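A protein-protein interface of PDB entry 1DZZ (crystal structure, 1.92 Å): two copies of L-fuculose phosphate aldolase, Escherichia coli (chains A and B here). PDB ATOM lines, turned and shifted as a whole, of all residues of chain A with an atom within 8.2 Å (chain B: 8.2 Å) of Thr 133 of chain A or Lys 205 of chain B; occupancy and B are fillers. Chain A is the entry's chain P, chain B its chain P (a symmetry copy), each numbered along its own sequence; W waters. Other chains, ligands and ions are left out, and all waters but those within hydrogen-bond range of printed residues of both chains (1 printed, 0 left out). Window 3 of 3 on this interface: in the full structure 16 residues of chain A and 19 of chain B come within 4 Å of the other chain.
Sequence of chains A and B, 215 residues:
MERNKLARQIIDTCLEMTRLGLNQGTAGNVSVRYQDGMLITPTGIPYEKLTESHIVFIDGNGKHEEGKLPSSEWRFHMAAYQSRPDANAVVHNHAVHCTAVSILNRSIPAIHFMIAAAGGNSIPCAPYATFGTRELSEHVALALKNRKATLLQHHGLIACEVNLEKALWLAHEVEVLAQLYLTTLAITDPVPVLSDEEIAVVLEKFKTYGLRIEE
Among the printed residues, pairs that only touch across the chains: Tyr 128 of chain A with Val 202 of chain B (3.9 Å), Thr 130 of chain A with Val 201 of chain B (3.9 Å), Thr 130 of chain A with Lys 205 of chain B (3.7 Å), Phe 131 of chain A with Phe 206 of chain B (3.6 Å) and Thr 133 of chain A with Lys 205 of chain B (3.8 Å).
Thr 133 of chain A touches one residue of chain B.
Printed residues of chain A within 4 Å of Lys 205 of chain B: Thr 130 (3.7 Å), Phe 131 (3.1 Å) and Thr 133 (3.8 Å).
Of the printed residues of chain B, Thr 130 of chain A touches Glu 198, Val 201 and Lys 205.
Of the printed residues of chain A, Val 202 of chain B touches Tyr 128.
Of the printed residues of chain B, Tyr 128 of chain A touches Glu 198 (2.7 Å) and Val 202 (3.9 Å).
Of the printed residues of chain A, Glu 198 of chain B touches Tyr 128 (2.7 Å) and Thr 130 (2.6 Å).
Glu 73 of chain A touches none of the printed residues of chain B.
Ile 199 of chain B touches none of the printed residues of chain A.
The nearest residue of chain B that does not touch Thr 133 of chain A is Val 201 of chain B (6.6 Å).
The nearest printed residue of chain B that does not touch Thr 130 of chain A is Val 202 of chain B (4.5 Å).
Water W1 lies within hydrogen-bond range of NZ of Lys 205 of chain B (2.8 Å) and O of Gly 132 of chain A (3.3 Å).
OG1 of Thr 133 of chain A sits at hydrogen-bond distance from N of Leu 136 of chain A, at 3.4 Å.
O of Thr 130 of chain A is in hydrogen-bond range of OG1 of Thr 133 of chain A (2.9 Å).
OH of Tyr 128 of chain A lies within hydrogen-bond range of OE2 of Glu 198 of chain B (2.7 Å).
The side-chain hydroxyl (OG1) of Thr 130 of chain A sits at hydrogen-bond distance from the side-chain carboxylate (OE2) of Glu 198 of chain B (2.6 Å).
O of Phe 131 of chain A is in hydrogen-bond range of NZ of Lys 205 of chain B, at 3.1 Å.
Hydrophobic or aromatic side chains of chain A that line the printed part of chain B: Tyr 128 and Phe 131.
Of the 11 printed residues of chain B, 5 touch a printed residue of chain A.
Among the printed residues, no Asp or Glu carboxylate lies within 4 Å of a Lys or Arg side-chain nitrogen of the other chain.
No position is printed for both chains.
Of the 8 pairs that touch across the chains among the printed residues, none has its exchanged pair printed and touching as well.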
ATOM      1  N   SER A  72      22.945   1.203  25.441  1.00  0.00           N
ATOM      2  CA  SER A  72      24.129   2.014  25.149  1.00  0.00           C
ATOM      3  C   SER A  72      24.211   3.258  26.007  1.00  0.00           C
ATOM      4  O   SER A  72      25.266   3.878  26.144  1.00  0.00           O
ATOM      5  CB  SER A  72      24.157   2.404  23.664  1.00  0.00           C
ATOM      6  OG  SER A  72      22.973   3.142  23.356  1.00  0.00           O
ATOM      7  N   GLU A  73      23.107   3.622  26.660  1.00  0.00           N
ATOM      8  CA  GLU A  73      23.001   4.771  27.522  1.00  0.00           C
ATOM      9  C   GLU A  73      22.999   4.474  29.007  1.00  0.00           C
ATOM     10  O   GLU A  73      22.592   5.329  29.792  1.00  0.00           O
ATOM     11  CB  GLU A  73      21.668   5.471  27.138  1.00  0.00           C
ATOM     12  CG  GLU A  73      21.595   5.633  25.617  1.00  0.00           C
ATOM     13  CD  GLU A  73      20.570   6.651  25.177  1.00  0.00           C
ATOM     14  OE1 GLU A  73      20.936   7.842  25.053  1.00  0.00           O
ATOM     15  OE2 GLU A  73      19.415   6.250  24.957  1.00  0.00           O
ATOM     16  N   TRP A  74      23.551   3.329  29.436  1.00  0.00           N
ATOM     17  CA  TRP A  74      23.536   2.985  30.847  1.00  0.00           C
ATOM     18  C   TRP A  74      24.288   3.993  31.696  1.00  0.00           C
ATOM     19  O   TRP A  74      23.924   4.231  32.861  1.00  0.00           O
ATOM     20  CB  TRP A  74      24.070   1.549  31.015  1.00  0.00           C
ATOM     21  CG  TRP A  74      25.554   1.401  30.808  1.00  0.00           C
ATOM     22  CD1 TRP A  74      26.162   0.987  29.649  1.00  0.00           C
ATOM     23  CD2 TRP A  74      26.608   1.683  31.740  1.00  0.00           C
ATOM     24  NE1 TRP A  74      27.523   0.999  29.812  1.00  0.00           N
ATOM     25  CE2 TRP A  74      27.829   1.424  31.082  1.00  0.00           C
ATOM     26  CE3 TRP A  74      26.637   2.134  33.056  1.00  0.00           C
ATOM     27  CZ2 TRP A  74      29.068   1.585  31.695  1.00  0.00           C
ATOM     28  CZ3 TRP A  74      27.859   2.302  33.678  1.00  0.00           C
ATOM     29  CH2 TRP A  74      29.065   2.027  32.998  1.00  0.00           C
ATOM     30  N   ARG A  75      25.378   4.613  31.213  1.00  0.00           N
ATOM     31  CA  ARG A  75      26.132   5.553  32.017  1.00  0.00           C
ATOM     32  C   ARG A  75      25.325   6.681  32.645  1.00  0.00           C
ATOM     33  O   ARG A  75      25.690   7.090  33.767  1.00  0.00           O
ATOM     34  CB  ARG A  75      27.296   6.189  31.255  1.00  0.00           C
ATOM     35  CG  ARG A  75      28.526   5.314  31.174  1.00  0.00           C
ATOM     36  CD  ARG A  75      29.602   6.037  30.358  1.00  0.00           C
ATOM     37  NE  ARG A  75      30.879   5.504  30.822  1.00  0.00           N
ATOM     38  CZ  ARG A  75      31.346   4.321  30.441  1.00  0.00           C
ATOM     39  NH1 ARG A  75      30.680   3.578  29.584  1.00  0.00           N
ATOM     40  NH2 ARG A  75      32.496   3.882  30.927  1.00  0.00           N
ATOM     41  N   PHE A  76      24.321   7.252  31.969  1.00  0.00           N
ATOM     42  CA  PHE A  76      23.583   8.336  32.630  1.00  0.00           C
ATOM     43  C   PHE A  76      22.526   7.755  33.571  1.00  0.00           C
ATOM     44  O   PHE A  76      22.060   8.505  34.424  1.00  0.00           O
ATOM     45  CB  PHE A  76      23.114   9.418  31.709  1.00  0.00           C
ATOM     46  CG  PHE A  76      22.134   9.129  30.613  1.00  0.00           C
ATOM     47  CD1 PHE A  76      20.985   8.390  30.856  1.00  0.00           C
ATOM     48  CD2 PHE A  76      22.338   9.645  29.339  1.00  0.00           C
ATOM     49  CE1 PHE A  76      20.071   8.135  29.847  1.00  0.00           C
ATOM     50  CE2 PHE A  76      21.411   9.398  28.336  1.00  0.00           C
ATOM     51  CZ  PHE A  76      20.291   8.631  28.580  1.00  0.00           C
ATOM     52  N   ALA A  79      24.583   7.719  36.607  1.00  0.00           N
ATOM     53  CA  ALA A  79      24.780   9.093  37.023  1.00  0.00           C
ATOM     54  C   ALA A  79      23.578   9.583  37.828  1.00  0.00           C
ATOM     55  O   ALA A  79      23.727  10.224  38.876  1.00  0.00           O
ATOM     56  CB  ALA A  79      24.995  10.037  35.840  1.00  0.00           C
ATOM     57  N   TYR A 128      23.849  19.552  25.154  1.00  0.00           N
ATOM     58  CA  TYR A 128      24.209  18.427  24.339  1.00  0.00           C
ATOM     59  C   TYR A 128      25.595  17.864  24.619  1.00  0.00           C
ATOM     60  O   TYR A 128      26.559  18.605  24.726  1.00  0.00           O
ATOM     61  CB  TYR A 128      24.113  18.786  22.821  1.00  0.00           C
ATOM     62  CG  TYR A 128      24.506  17.593  21.959  1.00  0.00           C
ATOM     63  CD1 TYR A 128      23.597  16.591  21.701  1.00  0.00           C
ATOM     64  CD2 TYR A 128      25.793  17.442  21.464  1.00  0.00           C
ATOM     65  CE1 TYR A 128      23.928  15.467  20.964  1.00  0.00           C
ATOM     66  CE2 TYR A 128      26.134  16.323  20.725  1.00  0.00           C
ATOM     67  CZ  TYR A 128      25.215  15.348  20.455  1.00  0.00           C
ATOM     68  OH  TYR A 128      25.513  14.233  19.724  1.00  0.00           O
ATOM     69  N   ALA A 129      25.733  16.547  24.582  1.00  0.00           N
ATOM     70  CA  ALA A 129      27.021  15.862  24.614  1.00  0.00           C
ATOM     71  C   ALA A 129      26.726  14.531  23.917  1.00  0.00           C
ATOM     72  O   ALA A 129      25.576  14.082  23.989  1.00  0.00           O
ATOM     73  CB  ALA A 129      27.583  15.636  25.994  1.00  0.00           C
ATOM     74  N   THR A 130      27.673  13.908  23.255  1.00  0.00           N
ATOM     75  CA  THR A 130      27.434  12.650  22.580  1.00  0.00           C
ATOM     76  C   THR A 130      26.822  11.594  23.485  1.00  0.00           C
ATOM     77  O   THR A 130      27.279  11.509  24.631  1.00  0.00           O
ATOM     78  CB  THR A 130      28.780  12.129  22.018  1.00  0.00           C
ATOM     79  OG1 THR A 130      29.331  13.167  21.207  1.00  0.00           O
ATOM     80  CG2 THR A 130      28.576  10.882  21.198  1.00  0.00           C
ATOM     81  N   PHE A 131      25.851  10.807  23.005  1.00  0.00           N
ATOM     82  CA  PHE A 131      25.256   9.754  23.830  1.00  0.00           C
ATOM     83  C   PHE A 131      26.326   8.793  24.351  1.00  0.00           C
ATOM     84  O   PHE A 131      27.364   8.570  23.705  1.00  0.00           O
ATOM     85  CB  PHE A 131      24.181   8.969  23.064  1.00  0.00           C
ATOM     86  CG  PHE A 131      24.680   8.065  21.967  1.00  0.00           C
ATOM     87  CD1 PHE A 131      24.931   8.565  20.699  1.00  0.00           C
ATOM     88  CD2 PHE A 131      24.915   6.725  22.203  1.00  0.00           C
ATOM     89  CE1 PHE A 131      25.407   7.742  19.690  1.00  0.00           C
ATOM     90  CE2 PHE A 131      25.388   5.898  21.193  1.00  0.00           C
ATOM     91  CZ  PHE A 131      25.634   6.401  19.925  1.00  0.00           C
ATOM     92  N   GLY A 132      26.097   8.210  25.532  1.00  0.00           N
ATOM     93  CA  GLY A 132      27.015   7.278  26.142  1.00  0.00           C
ATOM     94  C   GLY A 132      28.331   7.815  26.624  1.00  0.00           C
ATOM     95  O   GLY A 132      29.250   7.028  26.892  1.00  0.00           O
ATOM     96  N   THR A 133      28.538   9.120  26.774  1.00  0.00           N
ATOM     97  CA  THR A 133      29.848   9.609  27.212  1.00  0.00           C
ATOM     98  C   THR A 133      29.766  10.120  28.642  1.00  0.00           C
ATOM     99  O   THR A 133      28.682  10.352  29.191  1.00  0.00           O
ATOM    100  CB  THR A 133      30.383  10.720  26.294  1.00  0.00           C
ATOM    101  OG1 THR A 133      29.523  11.848  26.444  1.00  0.00           O
ATOM    102  CG2 THR A 133      30.416  10.250  24.838  1.00  0.00           C
ATOM    103  N   ARG A 134      30.950  10.328  29.211  1.00  0.00           N
ATOM    104  CA  ARG A 134      31.074  10.811  30.570  1.00  0.00           C
ATOM    105  C   ARG A 134      30.620  12.264  30.595  1.00  0.00           C
ATOM    106  O   ARG A 134      29.951  12.655  31.553  1.00  0.00           O
ATOM    107  CB  ARG A 134      32.490  10.653  31.130  1.00  0.00           C
ATOM    108  CG  ARG A 134      32.540   9.989  32.508  1.00  0.00           C
ATOM    109  CD  ARG A 134      31.882   8.606  32.510  1.00  0.00           C
ATOM    110  NE  ARG A 134      32.415   7.708  33.533  1.00  0.00           N
ATOM    111  CZ  ARG A 134      33.314   6.746  33.340  1.00  0.00           C
ATOM    112  NH1 ARG A 134      33.819   6.505  32.137  1.00  0.00           N
ATOM    113  NH2 ARG A 134      33.725   6.013  34.370  1.00  0.00           N
ATOM    114  N   GLU A 135      30.894  13.006  29.533  1.00  0.00           N
ATOM    115  CA  GLU A 135      30.471  14.394  29.456  1.00  0.00           C
ATOM    116  C   GLU A 135      28.952  14.488  29.602  1.00  0.00           C
ATOM    117  O   GLU A 135      28.457  15.288  30.386  1.00  0.00           O
ATOM    118  CB  GLU A 135      30.984  15.016  28.159  1.00  0.00           C
ATOM    119  CG  GLU A 135      31.410  16.461  28.269  1.00  0.00           C
ATOM    120  CD  GLU A 135      31.256  17.269  26.991  1.00  0.00           C
ATOM    121  OE1 GLU A 135      31.496  16.743  25.872  1.00  0.00           O
ATOM    122  OE2 GLU A 135      30.882  18.474  27.112  1.00  0.00           O
ATOM    123  N   LEU A 136      28.179  13.655  28.931  1.00  0.00           N
ATOM    124  CA  LEU A 136      26.718  13.656  29.019  1.00  0.00           C
ATOM    125  C   LEU A 136      26.250  13.364  30.447  1.00  0.00           C
ATOM    126  O   LEU A 136      25.349  14.019  30.974  1.00  0.00           O
ATOM    127  CB  LEU A 136      26.113  12.620  28.076  1.00  0.00           C
ATOM    128  CG  LEU A 136      24.842  12.904  27.293  1.00  0.00           C
ATOM    129  CD1 LEU A 136      24.042  11.626  27.046  1.00  0.00           C
ATOM    130  CD2 LEU A 136      23.994  14.029  27.853  1.00  0.00           C
ATOM    131  N   SER A 137      26.871  12.363  31.058  1.00  0.00           N
ATOM    132  CA  SER A 137      26.622  11.937  32.411  1.00  0.00           C
ATOM    133  C   SER A 137      26.757  13.086  33.394  1.00  0.00           C
ATOM    134  O   SER A 137      25.884  13.195  34.253  1.00  0.00           O
ATOM    135  CB  SER A 137      27.581  10.817  32.864  1.00  0.00           C
ATOM    136  OG  SER A 137      27.079   9.616  32.282  1.00  0.00           O
ATOM    137  N   GLU A 138      27.790  13.893  33.272  1.00  0.00           N
ATOM    138  CA  GLU A 138      27.998  15.020  34.173  1.00  0.00           C
ATOM    139  C   GLU A 138      26.929  16.098  34.026  1.00  0.00           C
ATOM    140  O   GLU A 138      26.392  16.629  35.016  1.00  0.00           O
ATOM    141  CB  GLU A 138      29.411  15.574  33.933  1.00  0.00           C
ATOM    142  CG  GLU A 138      30.501  14.788  34.655  1.00  0.00           C
ATOM    143  CD  GLU A 138      31.884  15.003  34.071  1.00  0.00           C
ATOM    144  OE1 GLU A 138      32.098  15.811  33.130  1.00  0.00           O
ATOM    145  OE2 GLU A 138      32.826  14.327  34.544  1.00  0.00           O
ATOM    146  N   HIS A 139      26.524  16.392  32.790  1.00  0.00           N
ATOM    147  CA  HIS A 139      25.420  17.346  32.597  1.00  0.00           C
ATOM    148  C   HIS A 139      24.132  16.813  33.240  1.00  0.00           C
ATOM    149  O   HIS A 139      23.378  17.594  33.813  1.00  0.00           O
ATOM    150  CB  HIS A 139      25.147  17.585  31.113  1.00  0.00           C
ATOM    151  CG  HIS A 139      26.249  18.324  30.413  1.00  0.00           C
ATOM    152  ND1 HIS A 139      26.590  18.040  29.096  1.00  0.00           N
ATOM    153  CD2 HIS A 139      27.085  19.301  30.858  1.00  0.00           C
ATOM    154  CE1 HIS A 139      27.593  18.821  28.738  1.00  0.00           C
ATOM    155  NE2 HIS A 139      27.903  19.588  29.785  1.00  0.00           N
ATOM    156  N   VAL A 140      23.821  15.538  33.071  1.00  0.00           N
ATOM    157  CA  VAL A 140      22.625  14.929  33.643  1.00  0.00           C
ATOM    158  C   VAL A 140      22.642  14.969  35.165  1.00  0.00           C
ATOM    159  O   VAL A 140      21.623  15.316  35.798  1.00  0.00           O
ATOM    160  CB  VAL A 140      22.491  13.484  33.122  1.00  0.00           C
ATOM    161  CG1 VAL A 140      21.521  12.605  33.893  1.00  0.00           C
ATOM    162  CG2 VAL A 140      22.067  13.565  31.655  1.00  0.00           C
ATOM    163  N   GLU B 198      30.031  16.768  14.940  1.00  0.00           N
ATOM    164  CA  GLU B 198      29.257  15.942  15.871  1.00  0.00           C
ATOM    165  C   GLU B 198      28.579  14.795  15.149  1.00  0.00           C
ATOM    166  O   GLU B 198      28.657  13.657  15.656  1.00  0.00           O
ATOM    167  CB  GLU B 198      28.255  16.733  16.709  1.00  0.00           C
ATOM    168  CG  GLU B 198      27.547  15.829  17.711  1.00  0.00           C
ATOM    169  CD  GLU B 198      28.445  15.074  18.683  1.00  0.00           C
ATOM    170  OE1 GLU B 198      29.483  15.663  19.095  1.00  0.00           O
ATOM    171  OE2 GLU B 198      28.118  13.915  19.019  1.00  0.00           O
ATOM    172  N   ILE B 199      27.972  14.987  13.969  1.00  0.00           N
ATOM    173  CA  ILE B 199      27.350  13.852  13.264  1.00  0.00           C
ATOM    174  C   ILE B 199      28.386  12.798  12.882  1.00  0.00           C
ATOM    175  O   ILE B 199      28.151  11.597  12.983  1.00  0.00           O
ATOM    176  CB  ILE B 199      26.534  14.289  12.035  1.00  0.00           C
ATOM    177  CG1 ILE B 199      25.337  15.126  12.524  1.00  0.00           C
ATOM    178  CG2 ILE B 199      26.085  13.098  11.193  1.00  0.00           C
ATOM    179  CD1 ILE B 199      24.260  14.365  13.268  1.00  0.00           C
ATOM    180  N   ALA B 200      29.616  13.251  12.588  1.00  0.00           N
ATOM    181  CA  ALA B 200      30.728  12.366  12.290  1.00  0.00           C
ATOM    182  C   ALA B 200      31.050  11.434  13.451  1.00  0.00           C
ATOM    183  O   ALA B 200      31.201  10.228  13.230  1.00  0.00           O
ATOM    184  CB  ALA B 200      31.942  13.224  11.912  1.00  0.00           C
ATOM    185  N   VAL B 201      31.071  11.942  14.680  1.00  0.00           N
ATOM    186  CA  VAL B 201      31.277  11.077  15.845  1.00  0.00           C
ATOM    187  C   VAL B 201      30.140  10.089  16.031  1.00  0.00           C
ATOM    188  O   VAL B 201      30.320   8.924  16.381  1.00  0.00           O
ATOM    189  CB  VAL B 201      31.385  11.927  17.121  1.00  0.00           C
ATOM    190  CG1 VAL B 201      31.328  11.094  18.398  1.00  0.00           C
ATOM    191  CG2 VAL B 201      32.690  12.729  17.109  1.00  0.00           C
ATOM    192  N   VAL B 202      28.893  10.555  15.856  1.00  0.00           N
ATOM    193  CA  VAL B 202      27.741   9.673  16.045  1.00  0.00           C
ATOM    194  C   VAL B 202      27.765   8.573  15.006  1.00  0.00           C
ATOM    195  O   VAL B 202      27.535   7.405  15.352  1.00  0.00           O
ATOM    196  CB  VAL B 202      26.443  10.493  16.017  1.00  0.00           C
ATOM    197  CG1 VAL B 202      25.222   9.580  15.945  1.00  0.00           C
ATOM    198  CG2 VAL B 202      26.397  11.349  17.292  1.00  0.00           C
ATOM    199  N   LEU B 203      28.104   8.897  13.752  1.00  0.00           N
ATOM    200  CA  LEU B 203      28.236   7.845  12.749  1.00  0.00           C
ATOM    201  C   LEU B 203      29.313   6.821  13.118  1.00  0.00           C
ATOM    202  O   LEU B 203      29.092   5.614  12.945  1.00  0.00           O
ATOM    203  CB  LEU B 203      28.561   8.434  11.391  1.00  0.00           C
ATOM    204  CG  LEU B 203      27.402   9.020  10.601  1.00  0.00           C
ATOM    205  CD1 LEU B 203      27.991   9.810   9.443  1.00  0.00           C
ATOM    206  CD2 LEU B 203      26.468   7.910  10.126  1.00  0.00           C
ATOM    207  N   GLU B 204      30.456   7.248  13.649  1.00  0.00           N
ATOM    208  CA  GLU B 204      31.470   6.261  14.036  1.00  0.00           C
ATOM    209  C   GLU B 204      30.951   5.409  15.188  1.00  0.00           C
ATOM    210  O   GLU B 204      31.141   4.187  15.173  1.00  0.00           O
ATOM    211  CB  GLU B 204      32.822   6.873  14.377  1.00  0.00           C
ATOM    212  CG  GLU B 204      33.992   5.962  13.961  1.00  0.00           C
ATOM    213  CD  GLU B 204      34.480   6.389  12.574  1.00  0.00           C
ATOM    214  OE1 GLU B 204      33.791   6.046  11.576  1.00  0.00           O
ATOM    215  OE2 GLU B 204      35.519   7.093  12.524  1.00  0.00           O
ATOM    216  N   LYS B 205      30.261   6.018  16.157  1.00  0.00           N
ATOM    217  CA  LYS B 205      29.716   5.251  17.268  1.00  0.00           C
ATOM    218  C   LYS B 205      28.680   4.267  16.764  1.00  0.00           C
ATOM    219  O   LYS B 205      28.702   3.120  17.216  1.00  0.00           O
ATOM    220  CB  LYS B 205      29.140   6.129  18.371  1.00  0.00           C
ATOM    221  CG  LYS B 205      30.192   6.706  19.294  1.00  0.00           C
ATOM    222  CD  LYS B 205      29.582   7.388  20.510  1.00  0.00           C
ATOM    223  CE  LYS B 205      29.464   6.420  21.679  1.00  0.00           C
ATOM    224  NZ  LYS B 205      29.949   7.044  22.944  1.00  0.00           N
ATOM    225  N   PHE B 206      27.841   4.621  15.793  1.00  0.00           N
ATOM    226  CA  PHE B 206      26.867   3.683  15.251  1.00  0.00           C
ATOM    227  C   PHE B 206      27.522   2.501  14.543  1.00  0.00           C
ATOM    228  O   PHE B 206      26.842   1.472  14.428  1.00  0.00           O
ATOM    229  CB  PHE B 206      25.855   4.343  14.315  1.00  0.00           C
ATOM    230  CG  PHE B 206      24.773   5.167  14.951  1.00  0.00           C
ATOM    231  CD1 PHE B 206      24.647   5.307  16.323  1.00  0.00           C
ATOM    232  CD2 PHE B 206      23.855   5.822  14.139  1.00  0.00           C
ATOM    233  CE1 PHE B 206      23.647   6.070  16.890  1.00  0.00           C
ATOM    234  CE2 PHE B 206      22.849   6.585  14.688  1.00  0.00           C
ATOM    235  CZ  PHE B 206      22.751   6.716  16.064  1.00  0.00           C
ATOM    236  N   LYS B 207      28.761   2.597  14.071  1.00  0.00           N
ATOM    237  CA  LYS B 207      29.434   1.445  13.469  1.00  0.00           C
ATOM    238  C   LYS B 207      29.839   0.471  14.580  1.00  0.00           C
ATOM    239  O   LYS B 207      29.655  -0.739  14.494  1.00  0.00           O
ATOM    240  CB  LYS B 207      30.671   1.857  12.686  1.00  0.00           C
ATOM    241  CG  LYS B 207      30.432   2.381  11.283  1.00  0.00           C
ATOM    242  CD  LYS B 207      31.633   3.207  10.836  1.00  0.00           C
ATOM    243  CE  LYS B 207      31.452   3.753   9.429  1.00  0.00           C
ATOM    244  NZ  LYS B 207      31.414   5.241   9.385  1.00  0.00           N
ATOM    245  N   THR B 208      30.377   1.009  15.664  1.00  0.00           N
ATOM    246  CA  THR B 208      30.820   0.303  16.854  1.00  0.00           C
ATOM    247  C   THR B 208      29.709  -0.412  17.603  1.00  0.00           C
ATOM    248  O   THR B 208      28.769  -0.992  17.019  1.00  0.00           O
ATOM    249  CB  THR B 208      31.465   1.343  17.816  1.00  0.00           C
ATOM    250  OG1 THR B 208      32.443   2.111  17.087  1.00  0.00           O
ATOM    251  CG2 THR B 208      32.129   0.707  19.025  1.00  0.00           C
HETATM  252  O   HOH W   1      29.633   4.730  24.570  1.00  0.00           O
